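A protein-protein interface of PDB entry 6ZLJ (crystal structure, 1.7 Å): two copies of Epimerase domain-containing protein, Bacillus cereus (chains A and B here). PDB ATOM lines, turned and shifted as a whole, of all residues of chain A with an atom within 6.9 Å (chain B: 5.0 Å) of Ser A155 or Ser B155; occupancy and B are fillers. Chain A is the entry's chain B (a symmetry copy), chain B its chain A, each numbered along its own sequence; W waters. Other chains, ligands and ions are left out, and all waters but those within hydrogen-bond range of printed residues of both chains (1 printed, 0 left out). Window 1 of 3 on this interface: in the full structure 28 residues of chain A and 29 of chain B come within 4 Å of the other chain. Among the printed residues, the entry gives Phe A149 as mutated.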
ATOM      1  N   ASN A 102      24.039  22.960 -26.184  1.00  0.00           N
ATOM      2  CA  ASN A 102      24.153  21.552 -25.726  1.00  0.00           C
ATOM      3  C   ASN A 102      24.287  21.489 -24.205  1.00  0.00           C
ATOM      4  O   ASN A 102      23.859  20.470 -23.625  1.00  0.00           O
ATOM      5  CB  ASN A 102      25.327  20.831 -26.385  1.00  0.00           C
ATOM      6  CG  ASN A 102      25.187  20.706 -27.894  1.00  0.00           C
ATOM      7  OD1 ASN A 102      24.165  21.074 -28.457  1.00  0.00           O
ATOM      8  ND2 ASN A 102      26.219  20.227 -28.562  1.00  0.00           N
ATOM      9  N   ILE A 103      24.940  22.471 -23.591  1.00  0.00           N
ATOM     10  CA  ILE A 103      25.142  22.532 -22.118  1.00  0.00           C
ATOM     11  C   ILE A 103      24.129  23.461 -21.465  1.00  0.00           C
ATOM     12  O   ILE A 103      23.390  22.954 -20.634  1.00  0.00           O
ATOM     13  CB  ILE A 103      26.596  22.878 -21.775  1.00  0.00           C
ATOM     14  CG1 ILE A 103      27.538  21.927 -22.522  1.00  0.00           C
ATOM     15  CG2 ILE A 103      26.807  22.846 -20.262  1.00  0.00           C
ATOM     16  CD1 ILE A 103      28.994  22.033 -22.124  1.00  0.00           C
ATOM     17  N   THR A 106      20.443  22.325 -21.774  1.00  0.00           N
ATOM     18  CA  THR A 106      20.122  21.112 -20.999  1.00  0.00           C
ATOM     19  C   THR A 106      19.984  21.513 -19.520  1.00  0.00           C
ATOM     20  O   THR A 106      19.022  21.083 -18.849  1.00  0.00           O
ATOM     21  CB  THR A 106      21.221  20.061 -21.200  1.00  0.00           C
ATOM     22  OG1 THR A 106      21.259  19.660 -22.572  1.00  0.00           O
ATOM     23  CG2 THR A 106      21.008  18.835 -20.342  1.00  0.00           C
ATOM     24  N   HIS A 123      16.614  12.011 -22.439  1.00  0.00           N
ATOM     25  CA  HIS A 123      17.693  12.856 -22.985  1.00  0.00           C
ATOM     26  C   HIS A 123      18.409  12.116 -24.115  1.00  0.00           C
ATOM     27  O   HIS A 123      18.897  10.959 -23.891  1.00  0.00           O
ATOM     28  CB  HIS A 123      18.648  13.241 -21.870  1.00  0.00           C
ATOM     29  CG  HIS A 123      19.738  14.125 -22.349  1.00  0.00           C
ATOM     30  ND1 HIS A 123      20.978  13.632 -22.779  1.00  0.00           N
ATOM     31  CD2 HIS A 123      19.810  15.459 -22.445  1.00  0.00           C
ATOM     32  CE1 HIS A 123      21.752  14.653 -23.116  1.00  0.00           C
ATOM     33  NE2 HIS A 123      21.067  15.777 -22.925  1.00  0.00           N
ATOM     34  N   VAL A 129      30.236  10.359 -27.481  1.00  0.00           N
ATOM     35  CA  VAL A 129      30.812  10.543 -26.119  1.00  0.00           C
ATOM     36  C   VAL A 129      31.909   9.487 -25.870  1.00  0.00           C
ATOM     37  O   VAL A 129      32.790   9.746 -25.041  1.00  0.00           O
ATOM     38  CB  VAL A 129      29.746  10.542 -25.014  1.00  0.00           C
ATOM     39  CG1 VAL A 129      28.632  11.583 -25.273  1.00  0.00           C
ATOM     40  CG2 VAL A 129      29.184   9.162 -24.785  1.00  0.00           C
ATOM     41  N   PHE A 149      32.609  18.727 -29.725  1.00  0.00           N
ATOM     42  CA  PHE A 149      31.171  18.393 -29.839  1.00  0.00           C
ATOM     43  C   PHE A 149      30.845  17.277 -28.842  1.00  0.00           C
ATOM     44  O   PHE A 149      29.912  17.392 -28.017  1.00  0.00           O
ATOM     45  CB  PHE A 149      30.820  17.927 -31.253  1.00  0.00           C
ATOM     46  CG  PHE A 149      29.559  17.103 -31.310  1.00  0.00           C
ATOM     47  CD1 PHE A 149      28.332  17.681 -31.006  1.00  0.00           C
ATOM     48  CD2 PHE A 149      29.592  15.749 -31.612  1.00  0.00           C
ATOM     49  CE1 PHE A 149      27.172  16.927 -31.036  1.00  0.00           C
ATOM     50  CE2 PHE A 149      28.425  14.998 -31.635  1.00  0.00           C
ATOM     51  CZ  PHE A 149      27.212  15.598 -31.374  1.00  0.00           C
ATOM     52  N   GLY A 150      31.651  16.221 -28.854  1.00  0.00           N
ATOM     53  CA  GLY A 150      31.401  15.071 -27.972  1.00  0.00           C
ATOM     54  C   GLY A 150      31.524  15.474 -26.522  1.00  0.00           C
ATOM     55  O   GLY A 150      30.770  14.954 -25.716  1.00  0.00           O
ATOM     56  N   VAL A 151      32.455  16.379 -26.187  1.00  0.00           N
ATOM     57  CA  VAL A 151      32.621  16.886 -24.801  1.00  0.00           C
ATOM     58  C   VAL A 151      31.292  17.526 -24.365  1.00  0.00           C
ATOM     59  O   VAL A 151      30.828  17.230 -23.261  1.00  0.00           O
ATOM     60  CB  VAL A 151      33.813  17.845 -24.632  1.00  0.00           C
ATOM     61  CG1 VAL A 151      33.900  18.403 -23.216  1.00  0.00           C
ATOM     62  CG2 VAL A 151      35.137  17.171 -24.989  1.00  0.00           C
ATOM     63  N   THR A 152      30.708  18.383 -25.196  1.00  0.00           N
ATOM     64  CA  THR A 152      29.477  19.100 -24.852  1.00  0.00           C
ATOM     65  C   THR A 152      28.332  18.108 -24.648  1.00  0.00           C
ATOM     66  O   THR A 152      27.533  18.353 -23.743  1.00  0.00           O
ATOM     67  CB  THR A 152      29.125  20.205 -25.854  1.00  0.00           C
ATOM     68  OG1 THR A 152      28.787  19.674 -27.123  1.00  0.00           O
ATOM     69  CG2 THR A 152      30.238  21.221 -25.935  1.00  0.00           C
ATOM     70  N   LYS A 153      28.210  17.087 -25.482  1.00  0.00           N
ATOM     71  CA  LYS A 153      27.100  16.120 -25.334  1.00  0.00           C
ATOM     72  C   LYS A 153      27.327  15.349 -24.030  1.00  0.00           C
ATOM     73  O   LYS A 153      26.362  15.009 -23.357  1.00  0.00           O
ATOM     74  CB  LYS A 153      27.012  15.234 -26.579  1.00  0.00           C
ATOM     75  CG  LYS A 153      26.485  15.950 -27.819  1.00  0.00           C
ATOM     76  CD  LYS A 153      25.025  16.409 -27.746  1.00  0.00           C
ATOM     77  CE  LYS A 153      24.009  15.269 -27.679  1.00  0.00           C
ATOM     78  NZ  LYS A 153      22.609  15.759 -27.787  1.00  0.00           N
ATOM     79  N   LEU A 154      28.568  15.027 -23.701  1.00  0.00           N
ATOM     80  CA  LEU A 154      28.801  14.220 -22.496  1.00  0.00           C
ATOM     81  C   LEU A 154      28.495  15.094 -21.270  1.00  0.00           C
ATOM     82  O   LEU A 154      27.934  14.603 -20.294  1.00  0.00           O
ATOM     83  CB  LEU A 154      30.241  13.691 -22.532  1.00  0.00           C
ATOM     84  CG  LEU A 154      30.640  12.843 -21.338  1.00  0.00           C
ATOM     85  CD1 LEU A 154      29.666  11.682 -21.136  1.00  0.00           C
ATOM     86  CD2 LEU A 154      32.062  12.335 -21.493  1.00  0.00           C
ATOM     87  N   SER A 155      28.795  16.389 -21.334  1.00  0.00           N
ATOM     88  CA  SER A 155      28.471  17.371 -20.271  1.00  0.00           C
ATOM     89  C   SER A 155      26.943  17.399 -20.030  1.00  0.00           C
ATOM     90  O   SER A 155      26.527  17.386 -18.857  1.00  0.00           O
ATOM     91  CB  SER A 155      29.085  18.714 -20.640  1.00  0.00           C
ATOM     92  OG  SER A 155      29.116  19.555 -19.511  1.00  0.00           O
ATOM     93  N   GLY A 156      26.158  17.300 -21.098  1.00  0.00           N
ATOM     94  CA  GLY A 156      24.683  17.201 -21.054  1.00  0.00           C
ATOM     95  C   GLY A 156      24.253  15.950 -20.314  1.00  0.00           C
ATOM     96  O   GLY A 156      23.423  16.044 -19.398  1.00  0.00           O
ATOM     97  N   GLU A 157      24.890  14.820 -20.592  1.00  0.00           N
ATOM     98  CA  GLU A 157      24.571  13.565 -19.864  1.00  0.00           C
ATOM     99  C   GLU A 157      24.863  13.794 -18.377  1.00  0.00           C
ATOM    100  O   GLU A 157      24.072  13.344 -17.540  1.00  0.00           O
ATOM    101  CB  GLU A 157      25.382  12.360 -20.354  1.00  0.00           C
ATOM    102  CG  GLU A 157      25.068  11.879 -21.766  1.00  0.00           C
ATOM    103  CD  GLU A 157      25.709  10.522 -22.082  1.00  0.00           C
ATOM    104  OE1 GLU A 157      26.102   9.828 -21.121  1.00  0.00           O
ATOM    105  OE2 GLU A 157      25.816  10.156 -23.287  1.00  0.00           O
ATOM    106  N   HIS A 158      26.029  14.347 -18.048  1.00  0.00           N
ATOM    107  CA  HIS A 158      26.453  14.498 -16.634  1.00  0.00           C
ATOM    108  C   HIS A 158      25.468  15.398 -15.884  1.00  0.00           C
ATOM    109  O   HIS A 158      25.183  15.105 -14.703  1.00  0.00           O
ATOM    110  CB  HIS A 158      27.907  14.944 -16.552  1.00  0.00           C
ATOM    111  CG  HIS A 158      28.834  13.828 -16.833  1.00  0.00           C
ATOM    112  ND1 HIS A 158      29.960  13.987 -17.607  1.00  0.00           N
ATOM    113  CD2 HIS A 158      28.839  12.547 -16.418  1.00  0.00           C
ATOM    114  CE1 HIS A 158      30.583  12.822 -17.700  1.00  0.00           C
ATOM    115  NE2 HIS A 158      29.948  11.943 -16.974  1.00  0.00           N
ATOM    116  N   LEU A 159      24.962  16.458 -16.515  1.00  0.00           N
ATOM    117  CA  LEU A 159      23.911  17.313 -15.910  1.00  0.00           C
ATOM    118  C   LEU A 159      22.672  16.483 -15.607  1.00  0.00           C
ATOM    119  O   LEU A 159      22.088  16.681 -14.514  1.00  0.00           O
ATOM    120  CB  LEU A 159      23.567  18.473 -16.844  1.00  0.00           C
ATOM    121  CG  LEU A 159      24.619  19.558 -16.879  1.00  0.00           C
ATOM    122  CD1 LEU A 159      24.401  20.486 -18.056  1.00  0.00           C
ATOM    123  CD2 LEU A 159      24.637  20.305 -15.560  1.00  0.00           C
ATOM    124  N   CYS A 160      22.256  15.618 -16.533  1.00  0.00           N
ATOM    125  CA  CYS A 160      21.110  14.710 -16.296  1.00  0.00           C
ATOM    126  C   CYS A 160      21.340  13.932 -15.005  1.00  0.00           C
ATOM    127  O   CYS A 160      20.430  13.871 -14.171  1.00  0.00           O
ATOM    128  CB  CYS A 160      20.846  13.764 -17.464  1.00  0.00           C
ATOM    129  SG  CYS A 160      20.107  14.635 -18.864  1.00  0.00           S
ATOM    130  N   ILE B 103      34.817  25.967 -18.803  1.00  0.00           N
ATOM    131  CA  ILE B 103      34.782  25.275 -20.127  1.00  0.00           C
ATOM    132  C   ILE B 103      35.363  26.173 -21.205  1.00  0.00           C
ATOM    133  O   ILE B 103      36.349  25.750 -21.793  1.00  0.00           O
ATOM    134  CB  ILE B 103      33.391  24.722 -20.472  1.00  0.00           C
ATOM    135  CG1 ILE B 103      32.875  23.850 -19.320  1.00  0.00           C
ATOM    136  CG2 ILE B 103      33.451  23.942 -21.782  1.00  0.00           C
ATOM    137  CD1 ILE B 103      31.470  23.294 -19.485  1.00  0.00           C
ATOM    138  N   VAL B 151      30.579  18.849 -13.036  1.00  0.00           N
ATOM    139  CA  VAL B 151      30.383  18.651 -14.499  1.00  0.00           C
ATOM    140  C   VAL B 151      31.319  19.582 -15.291  1.00  0.00           C
ATOM    141  O   VAL B 151      31.905  19.083 -16.298  1.00  0.00           O
ATOM    142  CB  VAL B 151      28.923  18.871 -14.924  1.00  0.00           C
ATOM    143  CG1 VAL B 151      28.789  18.859 -16.447  1.00  0.00           C
ATOM    144  CG2 VAL B 151      28.020  17.846 -14.273  1.00  0.00           C
ATOM    145  N   THR B 152      31.352  20.884 -14.984  1.00  0.00           N
ATOM    146  CA  THR B 152      32.138  21.857 -15.795  1.00  0.00           C
ATOM    147  C   THR B 152      33.628  21.511 -15.663  1.00  0.00           C
ATOM    148  O   THR B 152      34.361  21.611 -16.620  1.00  0.00           O
ATOM    149  CB  THR B 152      31.883  23.322 -15.418  1.00  0.00           C
ATOM    150  OG1 THR B 152      32.312  23.587 -14.080  1.00  0.00           O
ATOM    151  CG2 THR B 152      30.433  23.714 -15.570  1.00  0.00           C
ATOM    152  N   LYS B 153      34.074  21.128 -14.486  1.00  0.00           N
ATOM    153  CA  LYS B 153      35.505  20.744 -14.321  1.00  0.00           C
ATOM    154  C   LYS B 153      35.796  19.471 -15.127  1.00  0.00           C
ATOM    155  O   LYS B 153      36.863  19.374 -15.746  1.00  0.00           O
ATOM    156  CB  LYS B 153      35.824  20.608 -12.835  1.00  0.00           C
ATOM    157  CG  LYS B 153      35.922  21.920 -12.057  1.00  0.00           C
ATOM    158  CD  LYS B 153      37.017  22.860 -12.504  1.00  0.00           C
ATOM    159  CE  LYS B 153      38.386  22.353 -12.093  1.00  0.00           C
ATOM    160  NZ  LYS B 153      39.466  23.297 -12.433  1.00  0.00           N
ATOM    161  N   LEU B 154      34.891  18.493 -15.103  1.00  0.00           N
ATOM    162  CA  LEU B 154      35.121  17.238 -15.825  1.00  0.00           C
ATOM    163  C   LEU B 154      35.126  17.561 -17.329  1.00  0.00           C
ATOM    164  O   LEU B 154      35.966  17.011 -18.038  1.00  0.00           O
ATOM    165  CB  LEU B 154      34.084  16.195 -15.426  1.00  0.00           C
ATOM    166  CG  LEU B 154      34.175  14.895 -16.208  1.00  0.00           C
ATOM    167  CD1 LEU B 154      35.583  14.289 -16.082  1.00  0.00           C
ATOM    168  CD2 LEU B 154      33.115  13.901 -15.744  1.00  0.00           C
ATOM    169  N   SER B 155      34.304  18.509 -17.813  1.00  0.00           N
ATOM    170  CA  SER B 155      34.342  18.942 -19.235  1.00  0.00           C
ATOM    171  C   SER B 155      35.698  19.547 -19.597  1.00  0.00           C
ATOM    172  O   SER B 155      36.203  19.299 -20.725  1.00  0.00           O
ATOM    173  CB  SER B 155      33.227  19.911 -19.564  1.00  0.00           C
ATOM    174  OG  SER B 155      32.005  19.251 -19.304  1.00  0.00           O
ATOM    175  N   GLY B 156      36.289  20.313 -18.695  1.00  0.00           N
ATOM    176  CA  GLY B 156      37.617  20.869 -18.943  1.00  0.00           C
ATOM    177  C   GLY B 156      38.648  19.759 -19.087  1.00  0.00           C
ATOM    178  O   GLY B 156      39.488  19.874 -19.973  1.00  0.00           O
ATOM    179  N   GLU B 157      38.588  18.726 -18.255  1.00  0.00           N
ATOM    180  CA  GLU B 157      39.473  17.539 -18.392  1.00  0.00           C
ATOM    181  C   GLU B 157      39.275  16.910 -19.766  1.00  0.00           C
ATOM    182  O   GLU B 157      40.242  16.607 -20.415  1.00  0.00           O
ATOM    183  CB  GLU B 157      39.155  16.455 -17.366  1.00  0.00           C
ATOM    184  CG  GLU B 157      39.626  16.746 -15.957  1.00  0.00           C
ATOM    185  CD  GLU B 157      39.534  15.520 -15.038  1.00  0.00           C
ATOM    186  OE1 GLU B 157      39.476  14.377 -15.566  1.00  0.00           O
ATOM    187  OE2 GLU B 157      39.519  15.694 -13.789  1.00  0.00           O
ATOM    188  N   HIS B 158      38.022  16.741 -20.193  1.00  0.00           N
ATOM    189  CA  HIS B 158      37.728  16.090 -21.483  1.00  0.00           C
ATOM    190  C   HIS B 158      38.286  16.956 -22.617  1.00  0.00           C
ATOM    191  O   HIS B 158      38.821  16.362 -23.555  1.00  0.00           O
ATOM    192  CB  HIS B 158      36.249  15.788 -21.645  1.00  0.00           C
ATOM    193  CG  HIS B 158      35.754  14.693 -20.763  1.00  0.00           C
ATOM    194  ND1 HIS B 158      34.459  14.684 -20.270  1.00  0.00           N
ATOM    195  CD2 HIS B 158      36.381  13.619 -20.242  1.00  0.00           C
ATOM    196  CE1 HIS B 158      34.306  13.604 -19.516  1.00  0.00           C
ATOM    197  NE2 HIS B 158      35.477  12.944 -19.471  1.00  0.00           N
ATOM    198  N   LEU B 159      38.212  18.287 -22.525  1.00  0.00           N
ATOM    199  CA  LEU B 159      38.815  19.165 -23.566  1.00  0.00           C
ATOM    200  C   LEU B 159      40.327  18.905 -23.637  1.00  0.00           C
ATOM    201  O   LEU B 159      40.834  18.789 -24.740  1.00  0.00           O
ATOM    202  CB  LEU B 159      38.510  20.615 -23.257  1.00  0.00           C
ATOM    203  CG  LEU B 159      37.083  21.036 -23.598  1.00  0.00           C
ATOM    204  CD1 LEU B 159      36.799  22.415 -23.034  1.00  0.00           C
ATOM    205  CD2 LEU B 159      36.869  21.015 -25.091  1.00  0.00           C
HETATM  206  O   HOH W   1      32.195  16.573 -20.685  1.00  0.00           O
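The side-chain hydroxyl of Ser B155 sits at hydrogen-bond distance from the side-chain hydroxyl of Ser A155, 2.9 Å away.
The side-chain hydroxyl (OG) of Ser B155 lies within hydrogen-bond range of the backbone carbonyl oxygen (O) of Val B151, at 3.0 Å. The backbone carbonyl oxygen of Leu A154 is in hydrogen-bond range of a ring nitrogen (ND1) of His A158 (3.4 Å).
CD1 of Ile A103 touches CD1 of Ile B103, at 3.8 Å. CG1 of Val A151 touches O of Ser B155, at 3.5 Å. CB of His B158 touches CG2 of Val A151, at 3.8 Å. Leu A154 touches His B158 (CD2 to CE1, 3.2 Å). CG1 of Val B151 touches OG of Ser A155 (3.2 Å). CB of His A158 touches CG2 of Val B151, 3.7 Å away. Leu B154 touches His A158 (CD2 to CE1, 3.4 Å).
Printed residues of chain B within 4 Å of Ser A155: Val B151 (3.2 Å) and Ser B155 (2.9 Å). Of the printed residues of chain A, Ser B155 touches Val A151 and Ser A155. Of the printed residues of chain A, His B158 touches Val A151 (3.8 Å) and Leu A154 (3.2 Å). Of the printed residues of chain A, Leu B154 touches His A158 (3.4 Å). Of the printed residues of chain B, Val A151 touches Ser B155 (3.5 Å) and His B158 (3.8 Å). Of the printed residues of chain B, His A158 touches Val B151 and Leu B154. Printed residues of chain A within 4 Å of Val B151: Ser A155 (3.2 Å) and His A158 (3.7 Å). The nearest residue of chain B that does not touch Ser A155 is Ile B103 (4.4 Å).
Of the 10 printed residues of chain B, 5 touch a printed residue of chain A. Hydrophobic or aromatic side chains of chain B that line the printed part of chain A: Ile B103, Val B151, Leu B154 and His B158.
Ile B103 touches its own counterpart, Ile A103. Val A151 touches His B158, and with the chains exchanged His A158 touches Val B151. Leu A154 touches His B158, and with the chains exchanged His A158 touches Leu B154. Ser B155 touches its own counterpart, Ser A155. Of the 8 pairs that touch across the chains among the printed residues, 8 have their exchanged pair printed and touching as well.
Water W1 lies within hydrogen-bond range of a ring nitrogen (ND1) of His B158 (3.0 Å), the backbone carbonyl oxygen (O) of Val A151 (3.0 Å), the side-chain hydroxyl (OG) of Ser B155 (3.0 Å) and the backbone NH (N) of Ser A155 (3.5 Å).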
